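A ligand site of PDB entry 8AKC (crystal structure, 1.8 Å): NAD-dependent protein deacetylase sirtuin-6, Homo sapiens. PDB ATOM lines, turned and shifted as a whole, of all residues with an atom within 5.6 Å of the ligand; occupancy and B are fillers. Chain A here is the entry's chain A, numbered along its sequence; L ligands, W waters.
Water W1 lies within hydrogen-bond range of an oxygen (O2) of the ligand (2.6 Å), the side-chain amide oxygen (OD1) of Asn 108 (2.7 Å) and the backbone carbonyl oxygen (O) of Gln 107 (3.1 Å). Water W2 lies within hydrogen-bond range of O of Gly 48 (2.8 Å), N of Ala 52 (3.1 Å), OG1 of Thr 51 (3.2 Å), N3 of the ligand (3.4 Å) and O of Ile 49 (3.5 Å).
N of Ser 210 sits at hydrogen-bond distance from O6 of the ligand, at 3.2 Å. The backbone NH (N) of Gln 236 sits close to an oxygen (O4) of the ligand (3.4 Å). The guanidinium group (NH1) of Arg 59 is in salt-bridge range of an oxygen (O1) of the ligand, 2.7 Å away. N4 of the ligand lies within hydrogen-bond range of OG1 of Thr 51. OG1 of Thr 209 lies within hydrogen-bond range of O6 of the ligand (2.7 Å). N of Val 252 lies within hydrogen-bond range of N1 of the ligand (2.9 Å). N of Phe 58 lies within hydrogen-bond range of O5 of the ligand, 2.8 Å away. O8 of the ligand is in hydrogen-bond range of ND2 of Asn 234, 2.8 Å away. An oxygen (O10) of the ligand sits at hydrogen-bond distance from the backbone carbonyl oxygen (O) of Gln 107, 2.8 Å away. The backbone NH of Leu 235 is in hydrogen-bond range of a nitrogen (N2) of the ligand (3.3 Å). OG of Ser 210 sits at hydrogen-bond distance from O1 of the ligand. The backbone NH of Arg 59 lies within hydrogen-bond range of an oxygen (O5) of the ligand, at 2.8 Å. ND1 of His 127 is in hydrogen-bond range of O10 of the ligand, 2.6 Å away. An oxygen (O2) of the ligand is in hydrogen-bond range of the backbone NH (N) of Ala 47 (3.0 Å). NE1 of Trp 65 sits at hydrogen-bond distance from O3 of the ligand (3.2 Å). OE1 of Gln 236 sits at hydrogen-bond distance from O8 of the ligand, at 2.6 Å.
N4 of the ligand lies close to O of Gly 48 (3.3 Å). An oxygen (O11) of the ligand sits close to the backbone carbonyl oxygen of Gly 208, at 3.4 Å. Gly 46 touches the ligand (CA to O2, 3.1 Å). Asp 57 touches the ligand (OD2 to C5, 3.3 Å). OD1 of Asn 108 touches O2 of the ligand, 3.97 Å away. Trp 182 touches the ligand. Ile 213 touches the ligand. O of Gly 250 touches C1 of the ligand, at 3.3 Å. Tyr 251 touches the ligand. Hydrophobic or aromatic side chains that line the ligand: Ala 47, Phe 58, Trp 65, His 127, Trp 182, Ile 213, Leu 235, Tyr 251 and Val 252. 22 residues have an atom within 4 Å of the ligand: Gly 46, Ala 47, Gly 48, Thr 51, Asp 57, Phe 58, Arg 59, Trp 65, Gln 107, Asn 108, His 127, Trp 182, Gly 208, Thr 209, Ser 210, Ile 213, Asn 234, Leu 235, Gln 236, Gly 250, Tyr 251 and Val 252. The nearest printed residue that does not touch the ligand is Gly 60 (4.05 Å).
O of Gly 208 is in hydrogen-bond range of N of Ala 47 (3.2 Å). The backbone carbonyl oxygen (O) of Gln 107 is in hydrogen-bond range of a ring nitrogen (ND1) of His 127 (3.1 Å). NE2 of Gln 212 lies within hydrogen-bond range of OG of Ser 210, 3.2 Å away. The side-chain carboxylate (OD1) of Asp 57 lies within hydrogen-bond range of the backbone NH (N) of Gly 60 (3.1 Å). The backbone NH (N) of Gln 107 is in hydrogen-bond range of the backbone carbonyl oxygen (O) of Thr 45 (3.0 Å). The side-chain hydroxyl of Thr 209 lies within hydrogen-bond range of the side-chain amide nitrogen of Gln 107 (3.0 Å). The backbone carbonyl oxygen (O) of Gly 208 is in hydrogen-bond range of the backbone NH (N) of Gly 48, at 2.9 Å. O of Gln 236 lies within hydrogen-bond range of ND2 of Asn 234 (3.1 Å).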
ATOM      1  N   GLU A  16      -4.063  29.630  -9.812  1.00  0.00           N
ATOM      2  CA  GLU A  16      -4.572  28.242  -9.948  1.00  0.00           C
ATOM      3  C   GLU A  16      -3.466  27.338  -9.414  1.00  0.00           C
ATOM      4  O   GLU A  16      -2.309  27.733  -9.549  1.00  0.00           O
ATOM      5  CB  GLU A  16      -4.956  28.009 -11.399  1.00  0.00           C
ATOM      6  CG  GLU A  16      -6.134  28.858 -11.833  1.00  0.00           C
ATOM      7  CD  GLU A  16      -6.890  28.265 -12.989  1.00  0.00           C
ATOM      8  OE1 GLU A  16      -6.250  27.902 -13.984  1.00  0.00           O
ATOM      9  OE2 GLU A  16      -8.100  28.141 -12.888  1.00  0.00           O
ATOM     10  N   THR A  45     -21.544  22.687  -4.054  1.00  0.00           N
ATOM     11  CA  THR A  45     -21.139  23.090  -5.426  1.00  0.00           C
ATOM     12  C   THR A  45     -21.233  24.607  -5.609  1.00  0.00           C
ATOM     13  O   THR A  45     -22.224  25.242  -5.154  1.00  0.00           O
ATOM     14  CB  THR A  45     -21.921  22.309  -6.490  1.00  0.00           C
ATOM     15  OG1 THR A  45     -23.278  22.687  -6.377  1.00  0.00           O
ATOM     16  CG2 THR A  45     -21.740  20.811  -6.370  1.00  0.00           C
ATOM     17  N   GLY A  46     -20.275  25.160  -6.345  1.00  0.00           N
ATOM     18  CA  GLY A  46     -20.271  26.569  -6.764  1.00  0.00           C
ATOM     19  C   GLY A  46     -19.941  26.637  -8.243  1.00  0.00           C
ATOM     20  O   GLY A  46     -20.057  25.556  -8.901  1.00  0.00           O
ATOM     21  N   ALA A  47     -19.557  27.832  -8.694  1.00  0.00           N
ATOM     22  CA  ALA A  47     -19.543  28.248 -10.112  1.00  0.00           C
ATOM     23  C   ALA A  47     -18.526  27.397 -10.874  1.00  0.00           C
ATOM     24  O   ALA A  47     -18.705  27.227 -12.080  1.00  0.00           O
ATOM     25  CB  ALA A  47     -19.243  29.743 -10.246  1.00  0.00           C
ATOM     26  N   GLY A  48     -17.540  26.855 -10.187  1.00  0.00           N
ATOM     27  CA  GLY A  48     -16.443  26.117 -10.842  1.00  0.00           C
ATOM     28  C   GLY A  48     -16.942  24.840 -11.480  1.00  0.00           C
ATOM     29  O   GLY A  48     -16.327  24.395 -12.460  1.00  0.00           O
ATOM     30  N   ILE A  49     -18.068  24.263 -11.013  1.00  0.00           N
ATOM     31  CA  ILE A  49     -18.618  23.014 -11.647  1.00  0.00           C
ATOM     32  C   ILE A  49     -19.335  23.328 -12.972  1.00  0.00           C
ATOM     33  O   ILE A  49     -19.724  22.380 -13.677  1.00  0.00           O
ATOM     34  CB  ILE A  49     -19.495  22.169 -10.713  1.00  0.00           C
ATOM     35  CG1 ILE A  49     -20.923  22.706 -10.530  1.00  0.00           C
ATOM     36  CG2 ILE A  49     -18.809  21.876  -9.396  1.00  0.00           C
ATOM     37  CD1 ILE A  49     -21.870  21.592 -10.199  1.00  0.00           C
ATOM     38  N   THR A  51     -18.059  25.775 -15.310  1.00  0.00           N
ATOM     39  CA  THR A  51     -17.098  26.403 -16.241  1.00  0.00           C
ATOM     40  C   THR A  51     -16.905  25.519 -17.488  1.00  0.00           C
ATOM     41  O   THR A  51     -16.684  26.103 -18.589  1.00  0.00           O
ATOM     42  CB  THR A  51     -15.751  26.798 -15.617  1.00  0.00           C
ATOM     43  OG1 THR A  51     -15.125  25.653 -14.999  1.00  0.00           O
ATOM     44  CG2 THR A  51     -15.881  28.007 -14.707  1.00  0.00           C
ATOM     45  N   ALA A  52     -16.971  24.204 -17.366  1.00  0.00           N
ATOM     46  CA  ALA A  52     -16.681  23.266 -18.487  1.00  0.00           C
ATOM     47  C   ALA A  52     -17.910  23.152 -19.380  1.00  0.00           C
ATOM     48  O   ALA A  52     -17.839  22.439 -20.380  1.00  0.00           O
ATOM     49  CB  ALA A  52     -16.266  21.916 -17.977  1.00  0.00           C
ATOM     50  N   ASP A  57     -17.022  31.393 -14.047  1.00  0.00           N
ATOM     51  CA  ASP A  57     -17.199  31.470 -12.568  1.00  0.00           C
ATOM     52  C   ASP A  57     -17.134  32.937 -12.155  1.00  0.00           C
ATOM     53  O   ASP A  57     -17.237  33.803 -13.029  1.00  0.00           O
ATOM     54  CB  ASP A  57     -16.198  30.578 -11.839  1.00  0.00           C
ATOM     55  CG  ASP A  57     -14.741  30.944 -12.037  1.00  0.00           C
ATOM     56  OD1 ASP A  57     -14.450  32.062 -12.485  1.00  0.00           O
ATOM     57  OD2 ASP A  57     -13.904  30.088 -11.722  1.00  0.00           O
ATOM     58  N   PHE A  58     -16.985  33.218 -10.861  1.00  0.00           N
ATOM     59  CA  PHE A  58     -16.975  34.608 -10.359  1.00  0.00           C
ATOM     60  C   PHE A  58     -15.548  35.078 -10.004  1.00  0.00           C
ATOM     61  O   PHE A  58     -15.251  36.239 -10.311  1.00  0.00           O
ATOM     62  CB  PHE A  58     -17.913  34.763  -9.152  1.00  0.00           C
ATOM     63  CG  PHE A  58     -19.384  34.639  -9.472  1.00  0.00           C
ATOM     64  CD1 PHE A  58     -20.100  35.714  -9.950  1.00  0.00           C
ATOM     65  CD2 PHE A  58     -20.037  33.416  -9.326  1.00  0.00           C
ATOM     66  CE1 PHE A  58     -21.453  35.595 -10.247  1.00  0.00           C
ATOM     67  CE2 PHE A  58     -21.386  33.303  -9.610  1.00  0.00           C
ATOM     68  CZ  PHE A  58     -22.097  34.399 -10.068  1.00  0.00           C
ATOM     69  N   ARG A  59     -14.728  34.235  -9.362  1.00  0.00           N
ATOM     70  CA  ARG A  59     -13.449  34.680  -8.747  1.00  0.00           C
ATOM     71  C   ARG A  59     -12.262  33.898  -9.304  1.00  0.00           C
ATOM     72  O   ARG A  59     -11.161  34.133  -8.814  1.00  0.00           O
ATOM     73  CB  ARG A  59     -13.484  34.578  -7.220  1.00  0.00           C
ATOM     74  CG  ARG A  59     -14.475  35.563  -6.607  1.00  0.00           C
ATOM     75  CD  ARG A  59     -14.679  35.384  -5.125  1.00  0.00           C
ATOM     76  NE  ARG A  59     -15.878  36.102  -4.730  1.00  0.00           N
ATOM     77  CZ  ARG A  59     -17.127  35.622  -4.737  1.00  0.00           C
ATOM     78  NH1 ARG A  59     -17.375  34.358  -5.063  1.00  0.00           N
ATOM     79  NH2 ARG A  59     -18.131  36.422  -4.399  1.00  0.00           N
ATOM     80  N   GLY A  60     -12.472  33.054 -10.326  1.00  0.00           N
ATOM     81  CA  GLY A  60     -11.387  32.405 -11.095  1.00  0.00           C
ATOM     82  C   GLY A  60     -10.639  33.386 -11.994  1.00  0.00           C
ATOM     83  O   GLY A  60     -11.004  34.570 -12.086  1.00  0.00           O
ATOM     84  N   PRO A  61      -9.570  32.979 -12.727  1.00  0.00           N
ATOM     85  CA  PRO A  61      -8.758  33.972 -13.439  1.00  0.00           C
ATOM     86  C   PRO A  61      -9.562  34.778 -14.473  1.00  0.00           C
ATOM     87  O   PRO A  61      -9.243  35.999 -14.668  1.00  0.00           O
ATOM     88  CB  PRO A  61      -7.665  33.129 -14.132  1.00  0.00           C
ATOM     89  CG  PRO A  61      -7.595  31.872 -13.311  1.00  0.00           C
ATOM     90  CD  PRO A  61      -9.026  31.632 -12.854  1.00  0.00           C
ATOM     91  N   TRP A  65     -16.342  38.654 -11.515  1.00  0.00           N
ATOM     92  CA  TRP A  65     -15.743  39.662 -10.607  1.00  0.00           C
ATOM     93  C   TRP A  65     -14.271  39.954 -10.930  1.00  0.00           C
ATOM     94  O   TRP A  65     -13.875  41.144 -10.889  1.00  0.00           O
ATOM     95  CB  TRP A  65     -15.887  39.276  -9.134  1.00  0.00           C
ATOM     96  CG  TRP A  65     -17.272  39.025  -8.631  1.00  0.00           C
ATOM     97  CD1 TRP A  65     -17.553  38.275  -7.526  1.00  0.00           C
ATOM     98  CD2 TRP A  65     -18.535  39.549  -9.099  1.00  0.00           C
ATOM     99  NE1 TRP A  65     -18.898  38.252  -7.296  1.00  0.00           N
ATOM    100  CE2 TRP A  65     -19.524  39.016  -8.246  1.00  0.00           C
ATOM    101  CE3 TRP A  65     -18.928  40.410 -10.135  1.00  0.00           C
ATOM    102  CZ2 TRP A  65     -20.887  39.306  -8.401  1.00  0.00           C
ATOM    103  CZ3 TRP A  65     -20.275  40.678 -10.301  1.00  0.00           C
ATOM    104  CH2 TRP A  65     -21.238  40.120  -9.453  1.00  0.00           C
ATOM    105  N   GLN A 107     -24.622  27.007  -4.541  1.00  0.00           N
ATOM    106  CA  GLN A 107     -24.630  28.474  -4.638  1.00  0.00           C
ATOM    107  C   GLN A 107     -24.913  28.910  -6.080  1.00  0.00           C
ATOM    108  O   GLN A 107     -25.040  30.097  -6.362  1.00  0.00           O
ATOM    109  CB  GLN A 107     -23.262  28.944  -4.132  1.00  0.00           C
ATOM    110  CG  GLN A 107     -22.964  28.600  -2.667  1.00  0.00           C
ATOM    111  CD  GLN A 107     -21.530  28.968  -2.322  1.00  0.00           C
ATOM    112  OE1 GLN A 107     -21.166  30.155  -2.286  1.00  0.00           O
ATOM    113  NE2 GLN A 107     -20.698  27.962  -2.106  1.00  0.00           N
ATOM    114  N   ASN A 108     -25.047  27.952  -6.998  1.00  0.00           N
ATOM    115  CA  ASN A 108     -25.157  28.257  -8.444  1.00  0.00           C
ATOM    116  C   ASN A 108     -26.619  28.602  -8.748  1.00  0.00           C
ATOM    117  O   ASN A 108     -27.533  27.956  -8.187  1.00  0.00           O
ATOM    118  CB  ASN A 108     -24.679  27.106  -9.319  1.00  0.00           C
ATOM    119  CG  ASN A 108     -23.234  26.798  -9.019  1.00  0.00           C
ATOM    120  OD1 ASN A 108     -22.510  27.679  -8.544  1.00  0.00           O
ATOM    121  ND2 ASN A 108     -22.809  25.590  -9.322  1.00  0.00           N
ATOM    122  N   HIS A 127     -28.718  30.553  -3.522  1.00  0.00           N
ATOM    123  CA  HIS A 127     -28.649  31.890  -4.166  1.00  0.00           C
ATOM    124  C   HIS A 127     -29.762  32.043  -5.211  1.00  0.00           C
ATOM    125  O   HIS A 127     -29.824  33.105  -5.866  1.00  0.00           O
ATOM    126  CB  HIS A 127     -27.221  32.154  -4.708  1.00  0.00           C
ATOM    127  CG  HIS A 127     -26.161  32.008  -3.655  1.00  0.00           C
ATOM    128  ND1 HIS A 127     -24.766  32.019  -3.938  1.00  0.00           N
ATOM    129  CD2 HIS A 127     -26.257  31.961  -2.316  1.00  0.00           C
ATOM    130  CE1 HIS A 127     -24.127  31.882  -2.821  1.00  0.00           C
ATOM    131  NE2 HIS A 127     -25.010  31.870  -1.815  1.00  0.00           N
ATOM    132  N   TRP A 182     -27.385  41.450  -3.401  1.00  0.00           N
ATOM    133  CA  TRP A 182     -26.376  41.492  -2.308  1.00  0.00           C
ATOM    134  C   TRP A 182     -27.047  41.607  -0.918  1.00  0.00           C
ATOM    135  O   TRP A 182     -26.536  40.966   0.020  1.00  0.00           O
ATOM    136  CB  TRP A 182     -25.390  42.627  -2.557  1.00  0.00           C
ATOM    137  CG  TRP A 182     -24.434  42.343  -3.674  1.00  0.00           C
ATOM    138  CD1 TRP A 182     -24.515  42.820  -4.957  1.00  0.00           C
ATOM    139  CD2 TRP A 182     -23.275  41.480  -3.630  1.00  0.00           C
ATOM    140  NE1 TRP A 182     -23.480  42.305  -5.708  1.00  0.00           N
ATOM    141  CE2 TRP A 182     -22.717  41.486  -4.918  1.00  0.00           C
ATOM    142  CE3 TRP A 182     -22.681  40.683  -2.644  1.00  0.00           C
ATOM    143  CZ2 TRP A 182     -21.576  40.753  -5.236  1.00  0.00           C
ATOM    144  CZ3 TRP A 182     -21.552  39.962  -2.948  1.00  0.00           C
ATOM    145  CH2 TRP A 182     -21.005  39.988  -4.233  1.00  0.00           C
ATOM    146  N   GLY A 208     -15.636  23.186  -6.853  1.00  0.00           N
ATOM    147  CA  GLY A 208     -15.573  24.481  -7.549  1.00  0.00           C
ATOM    148  C   GLY A 208     -16.301  25.573  -6.806  1.00  0.00           C
ATOM    149  O   GLY A 208     -17.035  26.251  -7.430  1.00  0.00           O
ATOM    150  N   THR A 209     -16.081  25.749  -5.502  1.00  0.00           N
ATOM    151  CA  THR A 209     -16.466  26.970  -4.741  1.00  0.00           C
ATOM    152  C   THR A 209     -15.265  27.461  -3.925  1.00  0.00           C
ATOM    153  O   THR A 209     -14.608  26.632  -3.274  1.00  0.00           O
ATOM    154  CB  THR A 209     -17.662  26.658  -3.852  1.00  0.00           C
ATOM    155  OG1 THR A 209     -17.833  27.846  -3.082  1.00  0.00           O
ATOM    156  CG2 THR A 209     -17.466  25.457  -2.970  1.00  0.00           C
ATOM    157  N   SER A 210     -14.966  28.774  -3.944  1.00  0.00           N
ATOM    158  CA  SER A 210     -13.860  29.349  -3.145  1.00  0.00           C
ATOM    159  C   SER A 210     -14.308  29.543  -1.696  1.00  0.00           C
ATOM    160  O   SER A 210     -13.448  29.904  -0.874  1.00  0.00           O
ATOM    161  CB  SER A 210     -13.357  30.634  -3.772  1.00  0.00           C
ATOM    162  OG  SER A 210     -14.354  31.615  -3.714  1.00  0.00           O
ATOM    163  N   LEU A 211     -15.599  29.322  -1.412  1.00  0.00           N
ATOM    164  CA  LEU A 211     -16.169  29.222  -0.033  1.00  0.00           C
ATOM    165  C   LEU A 211     -16.070  30.568   0.690  1.00  0.00           C
ATOM    166  O   LEU A 211     -15.937  30.559   1.942  1.00  0.00           O
ATOM    167  CB  LEU A 211     -15.446  28.152   0.787  1.00  0.00           C
ATOM    168  CG  LEU A 211     -15.517  26.718   0.285  1.00  0.00           C
ATOM    169  CD1 LEU A 211     -14.533  25.825   1.029  1.00  0.00           C
ATOM    170  CD2 LEU A 211     -16.950  26.174   0.405  1.00  0.00           C
ATOM    171  N   GLN A 212     -16.216  31.665  -0.035  1.00  0.00           N
ATOM    172  CA  GLN A 212     -15.957  33.039   0.457  1.00  0.00           C
ATOM    173  C   GLN A 212     -17.252  33.712   0.914  1.00  0.00           C
ATOM    174  O   GLN A 212     -17.150  34.714   1.616  1.00  0.00           O
ATOM    175  CB  GLN A 212     -15.286  33.837  -0.648  1.00  0.00           C
ATOM    176  CG  GLN A 212     -13.858  33.431  -0.935  1.00  0.00           C
ATOM    177  CD  GLN A 212     -13.186  34.526  -1.724  1.00  0.00           C
ATOM    178  OE1 GLN A 212     -13.170  35.662  -1.305  1.00  0.00           O
ATOM    179  NE2 GLN A 212     -12.591  34.181  -2.869  1.00  0.00           N
ATOM    180  N   ILE A 213     -18.410  33.196   0.508  1.00  0.00           N
ATOM    181  CA  ILE A 213     -19.753  33.805   0.774  1.00  0.00           C
ATOM    182  C   ILE A 213     -20.284  33.193   2.069  1.00  0.00           C
ATOM    183  O   ILE A 213     -20.383  31.937   2.140  1.00  0.00           O
ATOM    184  CB  ILE A 213     -20.729  33.582  -0.414  1.00  0.00           C
ATOM    185  CG1 ILE A 213     -20.396  34.441  -1.639  1.00  0.00           C
ATOM    186  CG2 ILE A 213     -22.174  33.767   0.021  1.00  0.00           C
ATOM    187  CD1 ILE A 213     -20.663  35.928  -1.493  1.00  0.00           C
ATOM    188  N   VAL A 233     -12.450  20.328  -3.290  1.00  0.00           N
ATOM    189  CA  VAL A 233     -11.964  20.165  -4.693  1.00  0.00           C
ATOM    190  C   VAL A 233     -12.088  21.550  -5.327  1.00  0.00           C
ATOM    191  O   VAL A 233     -13.217  22.081  -5.449  1.00  0.00           O
ATOM    192  CB  VAL A 233     -12.710  19.079  -5.488  1.00  0.00           C
ATOM    193  CG1 VAL A 233     -12.119  18.942  -6.890  1.00  0.00           C
ATOM    194  CG2 VAL A 233     -12.783  17.727  -4.786  1.00  0.00           C
ATOM    195  N   ASN A 234     -10.949  22.143  -5.701  1.00  0.00           N
ATOM    196  CA  ASN A 234     -10.913  23.532  -6.236  1.00  0.00           C
ATOM    197  C   ASN A 234      -9.549  23.807  -6.868  1.00  0.00           C
ATOM    198  O   ASN A 234      -8.510  23.365  -6.265  1.00  0.00           O
ATOM    199  CB  ASN A 234     -11.238  24.554  -5.159  1.00  0.00           C
ATOM    200  CG  ASN A 234     -11.969  25.733  -5.767  1.00  0.00           C
ATOM    201  OD1 ASN A 234     -13.025  25.534  -6.355  1.00  0.00           O
ATOM    202  ND2 ASN A 234     -11.425  26.924  -5.620  1.00  0.00           N
ATOM    203  N   LEU A 235      -9.541  24.515  -8.006  1.00  0.00           N
ATOM    204  CA  LEU A 235      -8.293  24.836  -8.737  1.00  0.00           C
ATOM    205  C   LEU A 235      -7.511  25.931  -7.982  1.00  0.00           C
ATOM    206  O   LEU A 235      -6.287  25.887  -8.033  1.00  0.00           O
ATOM    207  CB  LEU A 235      -8.610  25.263 -10.171  1.00  0.00           C
ATOM    208  CG  LEU A 235      -8.897  24.130 -11.141  1.00  0.00           C
ATOM    209  CD1 LEU A 235      -9.401  24.678 -12.463  1.00  0.00           C
ATOM    210  CD2 LEU A 235      -7.677  23.243 -11.345  1.00  0.00           C
ATOM    211  N   GLN A 236      -8.233  26.830  -7.312  1.00  0.00           N
ATOM    212  CA  GLN A 236      -7.691  27.937  -6.507  1.00  0.00           C
ATOM    213  C   GLN A 236      -7.762  27.544  -5.031  1.00  0.00           C
ATOM    214  O   GLN A 236      -8.534  26.627  -4.641  1.00  0.00           O
ATOM    215  CB  GLN A 236      -8.516  29.222  -6.673  1.00  0.00           C
ATOM    216  CG  GLN A 236      -8.383  29.910  -8.018  1.00  0.00           C
ATOM    217  CD  GLN A 236      -9.285  31.120  -8.162  1.00  0.00           C
ATOM    218  OE1 GLN A 236     -10.447  31.168  -7.732  1.00  0.00           O
ATOM    219  NE2 GLN A 236      -8.756  32.150  -8.804  1.00  0.00           N
ATOM    220  N   PRO A 237      -7.020  28.289  -4.183  1.00  0.00           N
ATOM    221  CA  PRO A 237      -7.249  28.280  -2.734  1.00  0.00           C
ATOM    222  C   PRO A 237      -8.678  28.694  -2.392  1.00  0.00           C
ATOM    223  O   PRO A 237      -9.342  29.413  -3.126  1.00  0.00           O
ATOM    224  CB  PRO A 237      -6.275  29.366  -2.189  1.00  0.00           C
ATOM    225  CG  PRO A 237      -5.233  29.504  -3.278  1.00  0.00           C
ATOM    226  CD  PRO A 237      -6.000  29.289  -4.558  1.00  0.00           C
ATOM    227  N   GLY A 250      -7.405  20.226  -9.090  1.00  0.00           N
ATOM    228  CA  GLY A 250      -7.609  19.746 -10.473  1.00  0.00           C
ATOM    229  C   GLY A 250      -9.024  20.034 -10.947  1.00  0.00           C
ATOM    230  O   GLY A 250      -9.867  20.434 -10.115  1.00  0.00           O
ATOM    231  N   TYR A 251      -9.273  19.862 -12.243  1.00  0.00           N
ATOM    232  CA  TYR A 251     -10.610  20.028 -12.881  1.00  0.00           C
ATOM    233  C   TYR A 251     -11.579  19.053 -12.215  1.00  0.00           C
ATOM    234  O   TYR A 251     -11.211  17.845 -12.038  1.00  0.00           O
ATOM    235  CB  TYR A 251     -10.473  19.899 -14.404  1.00  0.00           C
ATOM    236  CG  TYR A 251      -9.563  20.921 -15.041  1.00  0.00           C
ATOM    237  CD1 TYR A 251      -9.996  22.216 -15.255  1.00  0.00           C
ATOM    238  CD2 TYR A 251      -8.288  20.591 -15.462  1.00  0.00           C
ATOM    239  CE1 TYR A 251      -9.185  23.163 -15.846  1.00  0.00           C
ATOM    240  CE2 TYR A 251      -7.446  21.526 -16.024  1.00  0.00           C
ATOM    241  CZ  TYR A 251      -7.896  22.828 -16.203  1.00  0.00           C
ATOM    242  OH  TYR A 251      -7.061  23.735 -16.775  1.00  0.00           O
ATOM    243  N   VAL A 252     -12.697  19.586 -11.700  1.00  0.00           N
ATOM    244  CA  VAL A 252     -13.753  18.836 -11.006  1.00  0.00           C
ATOM    245  C   VAL A 252     -14.213  17.689 -11.910  1.00  0.00           C
ATOM    246  O   VAL A 252     -14.390  16.639 -11.386  1.00  0.00           O
ATOM    247  CB  VAL A 252     -14.907  19.696 -10.482  1.00  0.00           C
ATOM    248  CG1 VAL A 252     -15.736  20.314 -11.605  1.00  0.00           C
ATOM    249  CG2 VAL A 252     -15.771  18.922  -9.522  1.00  0.00           C
ATOM    250  N   ASP A 253     -14.191  17.827 -13.236  1.00  0.00           N
ATOM    251  CA  ASP A 253     -14.685  16.761 -14.128  1.00  0.00           C
ATOM    252  C   ASP A 253     -13.704  15.589 -14.111  1.00  0.00           C
ATOM    253  O   ASP A 253     -14.227  14.427 -14.106  1.00  0.00           O
ATOM    254  CB  ASP A 253     -14.980  17.210 -15.555  1.00  0.00           C
ATOM    255  CG  ASP A 253     -16.283  17.948 -15.769  1.00  0.00           C
ATOM    256  OD1 ASP A 253     -17.162  17.943 -14.841  1.00  0.00           O
ATOM    257  OD2 ASP A 253     -16.445  18.526 -16.852  1.00  0.00           O
HETATM  258  N1  LIG L   1     -12.401  22.478 -11.666  1.00  0.00           N
HETATM  259  C1  LIG L   1     -12.108  22.884 -10.417  1.00  0.00           C
HETATM  260  N2  LIG L   1     -12.218  24.101  -9.872  1.00  0.00           N
HETATM  261  C2  LIG L   1     -12.689  24.978 -10.758  1.00  0.00           C
HETATM  262  C3  LIG L   1     -12.997  24.731 -12.079  1.00  0.00           C
HETATM  263  C4  LIG L   1     -12.864  23.405 -12.546  1.00  0.00           C
HETATM  264  N3  LIG L   1     -13.145  23.040 -13.787  1.00  0.00           N
HETATM  265  N4  LIG L   1     -13.431  25.890 -12.662  1.00  0.00           N
HETATM  266  C5  LIG L   1     -13.401  26.798 -11.718  1.00  0.00           C
HETATM  267  N5  LIG L   1     -12.917  26.320 -10.554  1.00  0.00           N
HETATM  268  P1  LIG L   1     -16.188  31.421  -7.233  1.00  0.00           P
HETATM  269  P2  LIG L   1     -18.672  30.475  -5.876  1.00  0.00           P
HETATM  270  C6  LIG L   1     -12.758  26.978  -9.284  1.00  0.00           C
HETATM  271  O1  LIG L   1     -15.994  32.255  -6.037  1.00  0.00           O
HETATM  272  O2  LIG L   1     -19.831  29.601  -6.338  1.00  0.00           O
HETATM  273  C7  LIG L   1     -21.011  35.251  -6.081  1.00  0.00           C
HETATM  274  O3  LIG L   1     -21.119  36.575  -5.646  1.00  0.00           O
HETATM  275  C8  LIG L   1     -12.104  28.369  -9.281  1.00  0.00           C
HETATM  276  O4  LIG L   1     -10.730  28.166  -9.115  1.00  0.00           O
HETATM  277  O5  LIG L   1     -15.954  31.877  -8.631  1.00  0.00           O
HETATM  278  O6  LIG L   1     -17.874  29.961  -4.744  1.00  0.00           O
HETATM  279  C9  LIG L   1     -22.358  34.521  -6.335  1.00  0.00           C
HETATM  280  O7  LIG L   1     -23.421  34.986  -5.509  1.00  0.00           O
HETATM  281  C10 LIG L   1     -12.832  29.102  -8.141  1.00  0.00           C
HETATM  282  O8  LIG L   1     -12.115  29.269  -6.944  1.00  0.00           O
HETATM  283  O9  LIG L   1     -17.727  30.881  -7.121  1.00  0.00           O
HETATM  284  C11 LIG L   1     -21.991  33.054  -6.097  1.00  0.00           C
HETATM  285  O10 LIG L   1     -23.098  32.135  -5.937  1.00  0.00           O
HETATM  286  C12 LIG L   1     -14.068  28.228  -7.827  1.00  0.00           C
HETATM  287  O11 LIG L   1     -14.049  27.170  -8.798  1.00  0.00           O
HETATM  288  C13 LIG L   1     -21.127  33.246  -4.855  1.00  0.00           C
HETATM  289  O12 LIG L   1     -20.363  34.463  -5.093  1.00  0.00           O
HETATM  290  C14 LIG L   1     -15.382  28.932  -7.938  1.00  0.00           C
HETATM  291  O13 LIG L   1     -15.375  30.064  -7.037  1.00  0.00           O
HETATM  292  C15 LIG L   1     -20.197  32.109  -4.509  1.00  0.00           C
HETATM  293  O14 LIG L   1     -19.243  31.916  -5.588  1.00  0.00           O
HETATM  294  O   HOH W   1     -22.135  30.172  -7.503  1.00  0.00           O
HETATM  295  O   HOH W   2     -16.395  22.711 -14.684  1.00  0.00           O
HETATM  296  O   HOH W   3     -14.229  20.588 -14.639  1.00  0.00           O
HETATM  297  O   HOH W   4     -25.473  34.648  -7.131  1.00  0.00           O
